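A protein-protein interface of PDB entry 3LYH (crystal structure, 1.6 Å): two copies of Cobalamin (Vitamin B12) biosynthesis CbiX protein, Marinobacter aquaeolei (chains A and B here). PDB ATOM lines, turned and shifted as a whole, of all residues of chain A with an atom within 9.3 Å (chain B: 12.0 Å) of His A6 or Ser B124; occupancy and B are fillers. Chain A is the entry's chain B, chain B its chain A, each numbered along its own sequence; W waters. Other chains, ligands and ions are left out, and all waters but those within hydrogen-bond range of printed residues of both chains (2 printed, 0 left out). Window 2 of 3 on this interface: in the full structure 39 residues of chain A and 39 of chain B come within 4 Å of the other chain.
The side-chain carboxylate of Glu B120 lies within salt-bridge range of the guanidinium group of Arg A98, at 2.7 Å. The side-chain hydroxyl (OG) of Ser B124 sits at hydrogen-bond distance from the side-chain hydroxyl (OG1) of Thr A66 (2.7 Å). OG of Ser B124 sits at hydrogen-bond distance from NH2 of Arg A98 (2.7 Å).
Water W2 bridges the side-chain carboxylate of Glu B120 (2.6 Å) and the backbone NH of Glu A101 (2.8 Å). Water W1 bridges O of Glu A101 and OE2 of Glu B120.
Among the printed residues, pairs that only touch across the chains: His A6 with Ser B124 (3.5 Å), Ile A8 with Val B117 (3.9 Å), Ile A8 with Leu B121 (3.7 Å), Ile A35 with Val B117 (3.6 Å), Ile A35 with Leu B121 (3.5 Å), Arg A98 with Arg B123 (3.9 Å) and Ala A100 with Glu B120 (3.6 Å).
Printed residues of chain B that touch a printed residue of chain A: Val B117, Glu B120, Leu B121, Arg B123 and Ser B124. Hydrophobic or aromatic side chains of chain B within 4 Å of the printed part of chain A: Val B117 and Leu B121. Among the printed residues, 10 pairs touch across the chains.
No position is printed for both chains.
NE2 of His A6 is in hydrogen-bond range of OG1 of Thr A66, at 2.5 Å. The backbone carbonyl oxygen (O) of Asn A37 sits at hydrogen-bond distance from the backbone NH (N) of Ile A8, 2.8 Å away. O of Ile A8 is in hydrogen-bond range of N of Ala A39, at 3.0 Å. N of Ile A9 is in hydrogen-bond range of O of Thr A66 (3.0 Å). N of Arg A98 sits at hydrogen-bond distance from O of Phe A65, 3.0 Å away. The backbone carbonyl oxygen (O) of Val A67 is in hydrogen-bond range of the backbone NH (N) of Ala A100, at 2.8 Å.
Pro A5 touches none of the printed residues of chain B. Of chain B, only Ser B124 (3.5 Å) comes within 4 Å of His A6. Ile A8 touches just these residues of chain B: Val B117 and Leu B121. Of the printed residues of chain B, Ile A35 touches Val B117 and Leu B121. No residue of chain B comes within 4 Å of Gln A64. No residue of chain B comes within 4 Å of Phe A65. Thr A66 touches one residue of chain B. Arg A98 touches just these residues of chain B: Glu B120, Arg B123 and Ser B124. Of the printed residues of chain B, Ala A100 touches Glu B120 (3.6 Å). Of the printed residues of chain A, Glu B120 touches Arg A98 (2.7 Å) and Ala A100 (3.6 Å). Arg B123 touches one residue of chain A. Ser B124 touches just these residues of chain A: His A6, Thr A66 and Arg A98. The nearest residue of chain B that does not touch His A6 is Leu B121 (4.1 Å). The nearest printed residue of chain A that does not touch Ser B124 is Phe A65 (5.7 Å).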
ATOM      1  N   GLN A   4     -15.139 -11.014 -28.451  1.00  0.00           N
ATOM      2  CA  GLN A   4     -14.916  -9.749 -29.205  1.00  0.00           C
ATOM      3  C   GLN A   4     -13.837  -9.910 -30.295  1.00  0.00           C
ATOM      4  O   GLN A   4     -12.688  -9.471 -30.095  1.00  0.00           O
ATOM      5  CB  GLN A   4     -14.560  -8.609 -28.235  1.00  0.00           C
ATOM      6  N   PRO A   5     -14.164 -10.610 -31.416  1.00  0.00           N
ATOM      7  CA  PRO A   5     -15.213 -11.631 -31.639  1.00  0.00           C
ATOM      8  C   PRO A   5     -14.646 -13.015 -31.324  1.00  0.00           C
ATOM      9  O   PRO A   5     -13.484 -13.289 -31.643  1.00  0.00           O
ATOM     10  CB  PRO A   5     -15.501 -11.538 -33.139  1.00  0.00           C
ATOM     11  CG  PRO A   5     -14.207 -11.128 -33.730  1.00  0.00           C
ATOM     12  CD  PRO A   5     -13.506 -10.247 -32.690  1.00  0.00           C
ATOM     13  N   HIS A   6     -15.472 -13.861 -30.715  1.00  0.00           N
ATOM     14  CA  HIS A   6     -15.028 -15.123 -30.156  1.00  0.00           C
ATOM     15  C   HIS A   6     -15.650 -16.273 -30.936  1.00  0.00           C
ATOM     16  O   HIS A   6     -16.895 -16.422 -31.017  1.00  0.00           O
ATOM     17  CB  HIS A   6     -15.427 -15.193 -28.702  1.00  0.00           C
ATOM     18  CG  HIS A   6     -14.680 -16.224 -27.934  1.00  0.00           C
ATOM     19  ND1 HIS A   6     -13.566 -15.915 -27.181  1.00  0.00           N
ATOM     20  CD2 HIS A   6     -14.860 -17.560 -27.823  1.00  0.00           C
ATOM     21  CE1 HIS A   6     -13.101 -17.024 -26.630  1.00  0.00           C
ATOM     22  NE2 HIS A   6     -13.882 -18.028 -26.990  1.00  0.00           N
ATOM     23  N   GLN A   7     -14.786 -17.084 -31.534  1.00  0.00           N
ATOM     24  CA  GLN A   7     -15.255 -18.175 -32.399  1.00  0.00           C
ATOM     25  C   GLN A   7     -15.528 -19.379 -31.549  1.00  0.00           C
ATOM     26  O   GLN A   7     -14.671 -19.783 -30.786  1.00  0.00           O
ATOM     27  CB  GLN A   7     -14.189 -18.542 -33.431  1.00  0.00           C
ATOM     28  CG  GLN A   7     -14.547 -19.739 -34.335  1.00  0.00           C
ATOM     29  CD  GLN A   7     -15.581 -19.436 -35.434  1.00  0.00           C
ATOM     30  OE1 GLN A   7     -16.439 -20.292 -35.761  1.00  0.00           O
ATOM     31  NE2 GLN A   7     -15.477 -18.261 -36.034  1.00  0.00           N
ATOM     32  N   ILE A   8     -16.711 -19.960 -31.690  1.00  0.00           N
ATOM     33  CA  ILE A   8     -17.019 -21.254 -31.107  1.00  0.00           C
ATOM     34  C   ILE A   8     -16.784 -22.321 -32.178  1.00  0.00           C
ATOM     35  O   ILE A   8     -17.232 -22.204 -33.310  1.00  0.00           O
ATOM     36  CB  ILE A   8     -18.488 -21.321 -30.653  1.00  0.00           C
ATOM     37  CG1 ILE A   8     -18.726 -20.415 -29.440  1.00  0.00           C
ATOM     38  CG2 ILE A   8     -18.922 -22.775 -30.364  1.00  0.00           C
ATOM     39  CD1 ILE A   8     -18.204 -21.046 -28.103  1.00  0.00           C
ATOM     40  N   ILE A   9     -16.055 -23.362 -31.798  1.00  0.00           N
ATOM     41  CA  ILE A   9     -15.874 -24.557 -32.607  1.00  0.00           C
ATOM     42  C   ILE A   9     -16.527 -25.706 -31.864  1.00  0.00           C
ATOM     43  O   ILE A   9     -16.078 -26.067 -30.758  1.00  0.00           O
ATOM     44  CB  ILE A   9     -14.389 -24.873 -32.882  1.00  0.00           C
ATOM     45  CG1 ILE A   9     -13.760 -23.684 -33.570  1.00  0.00           C
ATOM     46  CG2 ILE A   9     -14.272 -26.100 -33.818  1.00  0.00           C
ATOM     47  CD1 ILE A   9     -12.244 -23.797 -33.842  1.00  0.00           C
ATOM     48  N   ILE A  35     -26.128 -18.178 -33.635  1.00  0.00           N
ATOM     49  CA  ILE A  35     -25.145 -17.249 -33.100  1.00  0.00           C
ATOM     50  C   ILE A  35     -24.052 -17.040 -34.097  1.00  0.00           C
ATOM     51  O   ILE A  35     -23.838 -17.823 -35.044  1.00  0.00           O
ATOM     52  CB  ILE A  35     -24.614 -17.610 -31.680  1.00  0.00           C
ATOM     53  CG1 ILE A  35     -23.735 -18.852 -31.712  1.00  0.00           C
ATOM     54  CG2 ILE A  35     -25.775 -17.785 -30.711  1.00  0.00           C
ATOM     55  CD1 ILE A  35     -22.845 -19.012 -30.476  1.00  0.00           C
ATOM     56  N   GLU A  36     -23.447 -15.880 -33.977  1.00  0.00           N
ATOM     57  CA  GLU A  36     -22.362 -15.534 -34.859  1.00  0.00           C
ATOM     58  C   GLU A  36     -21.089 -16.292 -34.525  1.00  0.00           C
ATOM     59  O   GLU A  36     -20.846 -16.677 -33.370  1.00  0.00           O
ATOM     60  CB  GLU A  36     -22.118 -14.032 -34.845  1.00  0.00           C
ATOM     61  CG  GLU A  36     -23.309 -13.189 -35.300  1.00  0.00           C
ATOM     62  CD  GLU A  36     -23.759 -13.529 -36.707  1.00  0.00           C
ATOM     63  OE1 GLU A  36     -22.890 -13.662 -37.602  1.00  0.00           O
ATOM     64  OE2 GLU A  36     -24.965 -13.678 -36.942  1.00  0.00           O
ATOM     65  N   ASN A  37     -20.285 -16.561 -35.553  1.00  0.00           N
ATOM     66  CA  ASN A  37     -18.925 -17.108 -35.357  1.00  0.00           C
ATOM     67  C   ASN A  37     -18.945 -18.444 -34.622  1.00  0.00           C
ATOM     68  O   ASN A  37     -18.262 -18.630 -33.590  1.00  0.00           O
ATOM     69  CB  ASN A  37     -18.028 -16.117 -34.642  1.00  0.00           C
ATOM     70  CG  ASN A  37     -18.048 -14.745 -35.311  1.00  0.00           C
ATOM     71  OD1 ASN A  37     -17.843 -14.653 -36.520  1.00  0.00           O
ATOM     72  ND2 ASN A  37     -18.347 -13.682 -34.535  1.00  0.00           N
ATOM     73  N   ALA A  38     -19.786 -19.350 -35.120  1.00  0.00           N
ATOM     74  CA  ALA A  38     -19.860 -20.707 -34.585  1.00  0.00           C
ATOM     75  C   ALA A  38     -19.843 -21.708 -35.747  1.00  0.00           C
ATOM     76  O   ALA A  38     -20.467 -21.476 -36.759  1.00  0.00           O
ATOM     77  CB  ALA A  38     -21.109 -20.868 -33.629  1.00  0.00           C
ATOM     78  N   ALA A  39     -19.061 -22.789 -35.591  1.00  0.00           N
ATOM     79  CA  ALA A  39     -18.891 -23.767 -36.679  1.00  0.00           C
ATOM     80  C   ALA A  39     -18.643 -25.149 -36.099  1.00  0.00           C
ATOM     81  O   ALA A  39     -18.097 -25.265 -34.979  1.00  0.00           O
ATOM     82  CB  ALA A  39     -17.737 -23.362 -37.564  1.00  0.00           C
ATOM     83  N   ALA A  57     -11.370 -18.639 -39.597  1.00  0.00           N
ATOM     84  CA  ALA A  57     -11.740 -17.605 -38.644  1.00  0.00           C
ATOM     85  C   ALA A  57     -10.585 -16.585 -38.570  1.00  0.00           C
ATOM     86  O   ALA A  57     -10.825 -15.382 -38.514  1.00  0.00           O
ATOM     87  CB  ALA A  57     -12.041 -18.218 -37.279  1.00  0.00           C
ATOM     88  N   GLY A  61      -9.834 -12.458 -39.268  1.00  0.00           N
ATOM     89  CA  GLY A  61      -9.470 -11.647 -38.090  1.00  0.00           C
ATOM     90  C   GLY A  61      -9.788 -12.161 -36.689  1.00  0.00           C
ATOM     91  O   GLY A  61      -9.565 -11.440 -35.704  1.00  0.00           O
ATOM     92  N   VAL A  62     -10.313 -13.386 -36.574  1.00  0.00           N
ATOM     93  CA  VAL A  62     -10.635 -13.949 -35.272  1.00  0.00           C
ATOM     94  C   VAL A  62      -9.382 -14.560 -34.678  1.00  0.00           C
ATOM     95  O   VAL A  62      -8.667 -15.316 -35.339  1.00  0.00           O
ATOM     96  CB  VAL A  62     -11.745 -15.033 -35.335  1.00  0.00           C
ATOM     97  CG1 VAL A  62     -12.004 -15.597 -33.952  1.00  0.00           C
ATOM     98  CG2 VAL A  62     -13.019 -14.443 -35.933  1.00  0.00           C
ATOM     99  N   GLU A  63      -9.115 -14.193 -33.434  1.00  0.00           N
ATOM    100  CA  GLU A  63      -7.939 -14.648 -32.733  1.00  0.00           C
ATOM    101  C   GLU A  63      -8.246 -15.492 -31.485  1.00  0.00           C
ATOM    102  O   GLU A  63      -7.311 -16.107 -30.987  1.00  0.00           O
ATOM    103  CB  GLU A  63      -7.063 -13.445 -32.347  1.00  0.00           C
ATOM    104  CG  GLU A  63      -6.761 -12.508 -33.522  1.00  0.00           C
ATOM    105  CD  GLU A  63      -5.925 -13.148 -34.642  1.00  0.00           C
ATOM    106  OE1 GLU A  63      -5.200 -14.134 -34.395  1.00  0.00           O
ATOM    107  OE2 GLU A  63      -5.973 -12.629 -35.784  1.00  0.00           O
ATOM    108  N   GLN A  64      -9.504 -15.475 -31.001  1.00  0.00           N
ATOM    109  CA  GLN A  64      -9.908 -16.109 -29.727  1.00  0.00           C
ATOM    110  C   GLN A  64     -10.965 -17.163 -30.063  1.00  0.00           C
ATOM    111  O   GLN A  64     -11.939 -16.883 -30.784  1.00  0.00           O
ATOM    112  CB  GLN A  64     -10.516 -15.095 -28.752  1.00  0.00           C
ATOM    113  CG  GLN A  64      -9.550 -13.989 -28.276  1.00  0.00           C
ATOM    114  CD  GLN A  64      -8.509 -14.475 -27.294  1.00  0.00           C
ATOM    115  OE1 GLN A  64      -8.713 -15.472 -26.590  1.00  0.00           O
ATOM    116  NE2 GLN A  64      -7.378 -13.759 -27.231  1.00  0.00           N
ATOM    117  N   PHE A  65     -10.738 -18.380 -29.567  1.00  0.00           N
ATOM    118  CA  PHE A  65     -11.579 -19.530 -29.862  1.00  0.00           C
ATOM    119  C   PHE A  65     -11.933 -20.246 -28.578  1.00  0.00           C
ATOM    120  O   PHE A  65     -11.163 -20.206 -27.624  1.00  0.00           O
ATOM    121  CB  PHE A  65     -10.832 -20.525 -30.776  1.00  0.00           C
ATOM    122  CG  PHE A  65     -10.470 -19.955 -32.114  1.00  0.00           C
ATOM    123  CD1 PHE A  65      -9.361 -19.115 -32.243  1.00  0.00           C
ATOM    124  CD2 PHE A  65     -11.161 -20.314 -33.266  1.00  0.00           C
ATOM    125  CE1 PHE A  65      -9.024 -18.558 -33.498  1.00  0.00           C
ATOM    126  CE2 PHE A  65     -10.838 -19.797 -34.505  1.00  0.00           C
ATOM    127  CZ  PHE A  65      -9.748 -18.919 -34.638  1.00  0.00           C
ATOM    128  N   THR A  66     -13.076 -20.918 -28.588  1.00  0.00           N
ATOM    129  CA  THR A  66     -13.439 -21.892 -27.559  1.00  0.00           C
ATOM    130  C   THR A  66     -13.935 -23.131 -28.297  1.00  0.00           C
ATOM    131  O   THR A  66     -14.834 -23.036 -29.120  1.00  0.00           O
ATOM    132  CB  THR A  66     -14.493 -21.377 -26.573  1.00  0.00           C
ATOM    133  OG1 THR A  66     -13.945 -20.228 -25.889  1.00  0.00           O
ATOM    134  CG2 THR A  66     -14.910 -22.452 -25.548  1.00  0.00           C
ATOM    135  N   VAL A  67     -13.269 -24.244 -28.025  1.00  0.00           N
ATOM    136  CA  VAL A  67     -13.674 -25.587 -28.490  1.00  0.00           C
ATOM    137  C   VAL A  67     -14.615 -26.192 -27.495  1.00  0.00           C
ATOM    138  O   VAL A  67     -14.263 -26.349 -26.309  1.00  0.00           O
ATOM    139  CB  VAL A  67     -12.447 -26.484 -28.705  1.00  0.00           C
ATOM    140  CG1 VAL A  67     -12.854 -27.907 -29.068  1.00  0.00           C
ATOM    141  CG2 VAL A  67     -11.541 -25.906 -29.834  1.00  0.00           C
ATOM    142  N   VAL A  68     -15.818 -26.497 -27.972  1.00  0.00           N
ATOM    143  CA  VAL A  68     -16.883 -27.168 -27.178  1.00  0.00           C
ATOM    144  C   VAL A  68     -16.994 -28.610 -27.744  1.00  0.00           C
ATOM    145  O   VAL A  68     -17.542 -28.804 -28.849  1.00  0.00           O
ATOM    146  CB  VAL A  68     -18.246 -26.476 -27.293  1.00  0.00           C
ATOM    147  CG1 VAL A  68     -19.302 -27.202 -26.449  1.00  0.00           C
ATOM    148  CG2 VAL A  68     -18.168 -25.003 -26.859  1.00  0.00           C
ATOM    149  N   THR A  96      -5.352 -18.082 -29.532  1.00  0.00           N
ATOM    150  CA  THR A  96      -5.681 -18.561 -28.182  1.00  0.00           C
ATOM    151  C   THR A  96      -6.979 -19.387 -28.278  1.00  0.00           C
ATOM    152  O   THR A  96      -7.997 -18.898 -28.781  1.00  0.00           O
ATOM    153  CB  THR A  96      -5.857 -17.412 -27.199  1.00  0.00           C
ATOM    154  OG1 THR A  96      -4.658 -16.625 -27.200  1.00  0.00           O
ATOM    155  CG2 THR A  96      -6.098 -17.923 -25.756  1.00  0.00           C
ATOM    156  N   ILE A  97      -6.912 -20.635 -27.825  1.00  0.00           N
ATOM    157  CA  ILE A  97      -8.036 -21.573 -27.894  1.00  0.00           C
ATOM    158  C   ILE A  97      -8.265 -22.191 -26.525  1.00  0.00           C
ATOM    159  O   ILE A  97      -7.399 -22.918 -26.036  1.00  0.00           O
ATOM    160  CB  ILE A  97      -7.791 -22.699 -28.931  1.00  0.00           C
ATOM    161  CG1 ILE A  97      -7.333 -22.139 -30.266  1.00  0.00           C
ATOM    162  CG2 ILE A  97      -9.017 -23.679 -29.060  1.00  0.00           C
ATOM    163  CD1 ILE A  97      -6.769 -23.217 -31.239  1.00  0.00           C
ATOM    164  N   ARG A  98      -9.417 -21.881 -25.924  1.00  0.00           N
ATOM    165  CA  ARG A  98      -9.851 -22.509 -24.697  1.00  0.00           C
ATOM    166  C   ARG A  98     -10.544 -23.821 -25.043  1.00  0.00           C
ATOM    167  O   ARG A  98     -11.291 -23.883 -25.996  1.00  0.00           O
ATOM    168  CB  ARG A  98     -10.816 -21.615 -23.944  1.00  0.00           C
ATOM    169  CG  ARG A  98     -11.280 -22.207 -22.646  1.00  0.00           C
ATOM    170  CD  ARG A  98     -11.981 -21.181 -21.738  1.00  0.00           C
ATOM    171  NE  ARG A  98     -13.357 -20.881 -22.127  1.00  0.00           N
ATOM    172  CZ  ARG A  98     -14.429 -21.629 -21.820  1.00  0.00           C
ATOM    173  NH1 ARG A  98     -14.313 -22.768 -21.118  1.00  0.00           N
ATOM    174  NH2 ARG A  98     -15.632 -21.230 -22.214  1.00  0.00           N
ATOM    175  N   LEU A  99     -10.300 -24.844 -24.240  1.00  0.00           N
ATOM    176  CA  LEU A  99     -10.965 -26.134 -24.373  1.00  0.00           C
ATOM    177  C   LEU A  99     -12.030 -26.217 -23.280  1.00  0.00           C
ATOM    178  O   LEU A  99     -11.711 -26.291 -22.091  1.00  0.00           O
ATOM    179  CB  LEU A  99      -9.919 -27.252 -24.258  1.00  0.00           C
ATOM    180  CG  LEU A  99     -10.457 -28.683 -24.203  1.00  0.00           C
ATOM    181  CD1 LEU A  99     -11.316 -28.915 -25.450  1.00  0.00           C
ATOM    182  CD2 LEU A  99      -9.365 -29.699 -24.053  1.00  0.00           C
ATOM    183  N   ALA A 100     -13.303 -26.115 -23.669  1.00  0.00           N
ATOM    184  CA  ALA A 100     -14.412 -26.274 -22.747  1.00  0.00           C
ATOM    185  C   ALA A 100     -14.608 -27.738 -22.370  1.00  0.00           C
ATOM    186  O   ALA A 100     -14.111 -28.635 -23.068  1.00  0.00           O
ATOM    187  CB  ALA A 100     -15.683 -25.698 -23.378  1.00  0.00           C
ATOM    188  N   GLU A 101     -15.334 -27.989 -21.267  1.00  0.00           N
ATOM    189  CA  GLU A 101     -15.748 -29.345 -20.899  1.00  0.00           C
ATOM    190  C   GLU A 101     -16.642 -29.934 -22.016  1.00  0.00           C
ATOM    191  O   GLU A 101     -17.342 -29.188 -22.695  1.00  0.00           O
ATOM    192  CB  GLU A 101     -16.466 -29.358 -19.515  1.00  0.00           C
ATOM    193  CG  GLU A 101     -17.892 -28.759 -19.502  1.00  0.00           C
ATOM    194  CD  GLU A 101     -18.566 -28.656 -18.111  1.00  0.00           C
ATOM    195  OE1 GLU A 101     -17.903 -29.057 -17.114  1.00  0.00           O
ATOM    196  OE2 GLU A 101     -19.750 -28.154 -18.050  1.00  0.00           O
ATOM    197  N   ARG B 114     -26.964 -25.465 -28.065  1.00  0.00           N
ATOM    198  CA  ARG B 114     -26.959 -24.003 -28.155  1.00  0.00           C
ATOM    199  C   ARG B 114     -26.960 -23.314 -26.778  1.00  0.00           C
ATOM    200  O   ARG B 114     -26.171 -22.405 -26.573  1.00  0.00           O
ATOM    201  CB  ARG B 114     -28.141 -23.516 -28.980  1.00  0.00           C
ATOM    202  CG  ARG B 114     -28.077 -22.037 -29.217  1.00  0.00           C
ATOM    203  CD  ARG B 114     -29.198 -21.481 -29.976  1.00  0.00           C
ATOM    204  NE  ARG B 114     -30.459 -21.798 -29.313  1.00  0.00           N
ATOM    205  CZ  ARG B 114     -31.623 -21.973 -29.931  1.00  0.00           C
ATOM    206  NH1 ARG B 114     -31.729 -21.912 -31.260  1.00  0.00           N
ATOM    207  NH2 ARG B 114     -32.694 -22.256 -29.199  1.00  0.00           N
ATOM    208  N   ASP B 115     -27.780 -23.808 -25.841  1.00  0.00           N
ATOM    209  CA  ASP B 115     -27.808 -23.274 -24.475  1.00  0.00           C
ATOM    210  C   ASP B 115     -26.463 -23.429 -23.775  1.00  0.00           C
ATOM    211  O   ASP B 115     -25.994 -22.529 -23.044  1.00  0.00           O
ATOM    212  CB  ASP B 115     -28.912 -23.945 -23.613  1.00  0.00           C
ATOM    213  CG  ASP B 115     -30.350 -23.679 -24.116  1.00  0.00           C
ATOM    214  OD1 ASP B 115     -30.581 -22.682 -24.823  1.00  0.00           O
ATOM    215  OD2 ASP B 115     -31.258 -24.507 -23.798  1.00  0.00           O
ATOM    216  N   VAL B 116     -25.815 -24.579 -23.974  1.00  0.00           N
ATOM    217  CA  VAL B 116     -24.523 -24.813 -23.391  1.00  0.00           C
ATOM    218  C   VAL B 116     -23.478 -23.870 -23.990  1.00  0.00           C
ATOM    219  O   VAL B 116     -22.618 -23.330 -23.274  1.00  0.00           O
ATOM    220  CB  VAL B 116     -24.102 -26.302 -23.547  1.00  0.00           C
ATOM    221  CG1 VAL B 116     -22.671 -26.494 -23.131  1.00  0.00           C
ATOM    222  CG2 VAL B 116     -25.051 -27.221 -22.687  1.00  0.00           C
ATOM    223  N   VAL B 117     -23.552 -23.669 -25.304  1.00  0.00           N
ATOM    224  CA  VAL B 117     -22.649 -22.784 -26.002  1.00  0.00           C
ATOM    225  C   VAL B 117     -22.764 -21.361 -25.441  1.00  0.00           C
ATOM    226  O   VAL B 117     -21.773 -20.658 -25.212  1.00  0.00           O
ATOM    227  CB  VAL B 117     -22.874 -22.865 -27.556  1.00  0.00           C
ATOM    228  CG1 VAL B 117     -22.164 -21.687 -28.221  1.00  0.00           C
ATOM    229  CG2 VAL B 117     -22.316 -24.191 -28.098  1.00  0.00           C
ATOM    230  N   LYS B 118     -24.005 -20.933 -25.210  1.00  0.00           N
ATOM    231  CA  LYS B 118     -24.236 -19.586 -24.678  1.00  0.00           C
ATOM    232  C   LYS B 118     -23.619 -19.424 -23.299  1.00  0.00           C
ATOM    233  O   LYS B 118     -23.076 -18.363 -22.988  1.00  0.00           O
ATOM    234  CB  LYS B 118     -25.716 -19.262 -24.648  1.00  0.00           C
ATOM    235  CG  LYS B 118     -26.265 -18.950 -26.004  1.00  0.00           C
ATOM    236  CD  LYS B 118     -27.715 -18.590 -25.916  1.00  0.00           C
ATOM    237  CE  LYS B 118     -28.250 -18.259 -27.264  1.00  0.00           C
ATOM    238  NZ  LYS B 118     -29.654 -17.822 -27.129  1.00  0.00           N
ATOM    239  N   GLU B 119     -23.721 -20.477 -22.492  1.00  0.00           N
ATOM    240  CA  GLU B 119     -23.062 -20.517 -21.176  1.00  0.00           C
ATOM    241  C   GLU B 119     -21.557 -20.419 -21.289  1.00  0.00           C
ATOM    242  O   GLU B 119     -20.912 -19.661 -20.535  1.00  0.00           O
ATOM    243  CB  GLU B 119     -23.423 -21.805 -20.421  1.00  0.00           C
ATOM    244  CG  GLU B 119     -24.721 -21.847 -19.724  1.00  0.00           C
ATOM    245  CD  GLU B 119     -24.914 -23.156 -18.929  1.00  0.00           C
ATOM    246  OE1 GLU B 119     -23.935 -23.877 -18.676  1.00  0.00           O
ATOM    247  OE2 GLU B 119     -26.060 -23.462 -18.573  1.00  0.00           O
ATOM    248  N   GLU B 120     -20.987 -21.155 -22.245  1.00  0.00           N
ATOM    249  CA  GLU B 120     -19.543 -21.127 -22.480  1.00  0.00           C
ATOM    250  C   GLU B 120     -19.029 -19.782 -23.006  1.00  0.00           C
ATOM    251  O   GLU B 120     -17.900 -19.387 -22.681  1.00  0.00           O
ATOM    252  CB  GLU B 120     -19.091 -22.231 -23.425  1.00  0.00           C
ATOM    253  CG  GLU B 120     -19.229 -23.618 -22.859  1.00  0.00           C
ATOM    254  CD  GLU B 120     -18.306 -23.904 -21.685  1.00  0.00           C
ATOM    255  OE1 GLU B 120     -17.454 -23.074 -21.323  1.00  0.00           O
ATOM    256  OE2 GLU B 120     -18.481 -25.006 -21.104  1.00  0.00           O
ATOM    257  N   LEU B 121     -19.840 -19.088 -23.812  1.00  0.00           N
ATOM    258  CA  LEU B 121     -19.495 -17.735 -24.260  1.00  0.00           C
ATOM    259  C   LEU B 121     -19.464 -16.740 -23.094  1.00  0.00           C
ATOM    260  O   LEU B 121     -18.633 -15.811 -23.086  1.00  0.00           O
ATOM    261  CB  LEU B 121     -20.455 -17.261 -25.360  1.00  0.00           C
ATOM    262  CG  LEU B 121     -20.218 -17.905 -26.737  1.00  0.00           C
ATOM    263  CD1 LEU B 121     -21.389 -17.683 -27.637  1.00  0.00           C
ATOM    264  CD2 LEU B 121     -18.944 -17.370 -27.410  1.00  0.00           C
ATOM    265  N   GLU B 122     -20.356 -16.932 -22.137  1.00  0.00           N
ATOM    266  CA  GLU B 122     -20.408 -16.066 -20.956  1.00  0.00           C
ATOM    267  C   GLU B 122     -19.153 -16.287 -20.092  1.00  0.00           C
ATOM    268  O   GLU B 122     -18.599 -15.321 -19.545  1.00  0.00           O
ATOM    269  CB  GLU B 122     -21.705 -16.287 -20.170  1.00  0.00           C
ATOM    270  N   ARG B 123     -18.699 -17.541 -19.992  1.00  0.00           N
ATOM    271  CA  ARG B 123     -17.401 -17.875 -19.370  1.00  0.00           C
ATOM    272  C   ARG B 123     -16.191 -17.316 -20.147  1.00  0.00           C
ATOM    273  O   ARG B 123     -15.255 -16.807 -19.547  1.00  0.00           O
ATOM    274  CB  ARG B 123     -17.257 -19.404 -19.234  1.00  0.00           C
ATOM    275  N   SER B 124     -16.213 -17.415 -21.475  1.00  0.00           N
ATOM    276  CA  SER B 124     -15.049 -17.045 -22.318  1.00  0.00           C
ATOM    277  C   SER B 124     -14.784 -15.536 -22.400  1.00  0.00           C
ATOM    278  O   SER B 124     -15.579 -14.722 -21.924  1.00  0.00           O
ATOM    279  CB  SER B 124     -15.215 -17.617 -23.733  1.00  0.00           C
ATOM    280  OG  SER B 124     -15.140 -19.041 -23.719  1.00  0.00           O
HETATM  281  O   HOH W   1     -19.325 -27.415 -22.621  1.00  0.00           O
HETATM  282  O   HOH W   2     -16.258 -25.700 -19.903  1.00  0.00           O
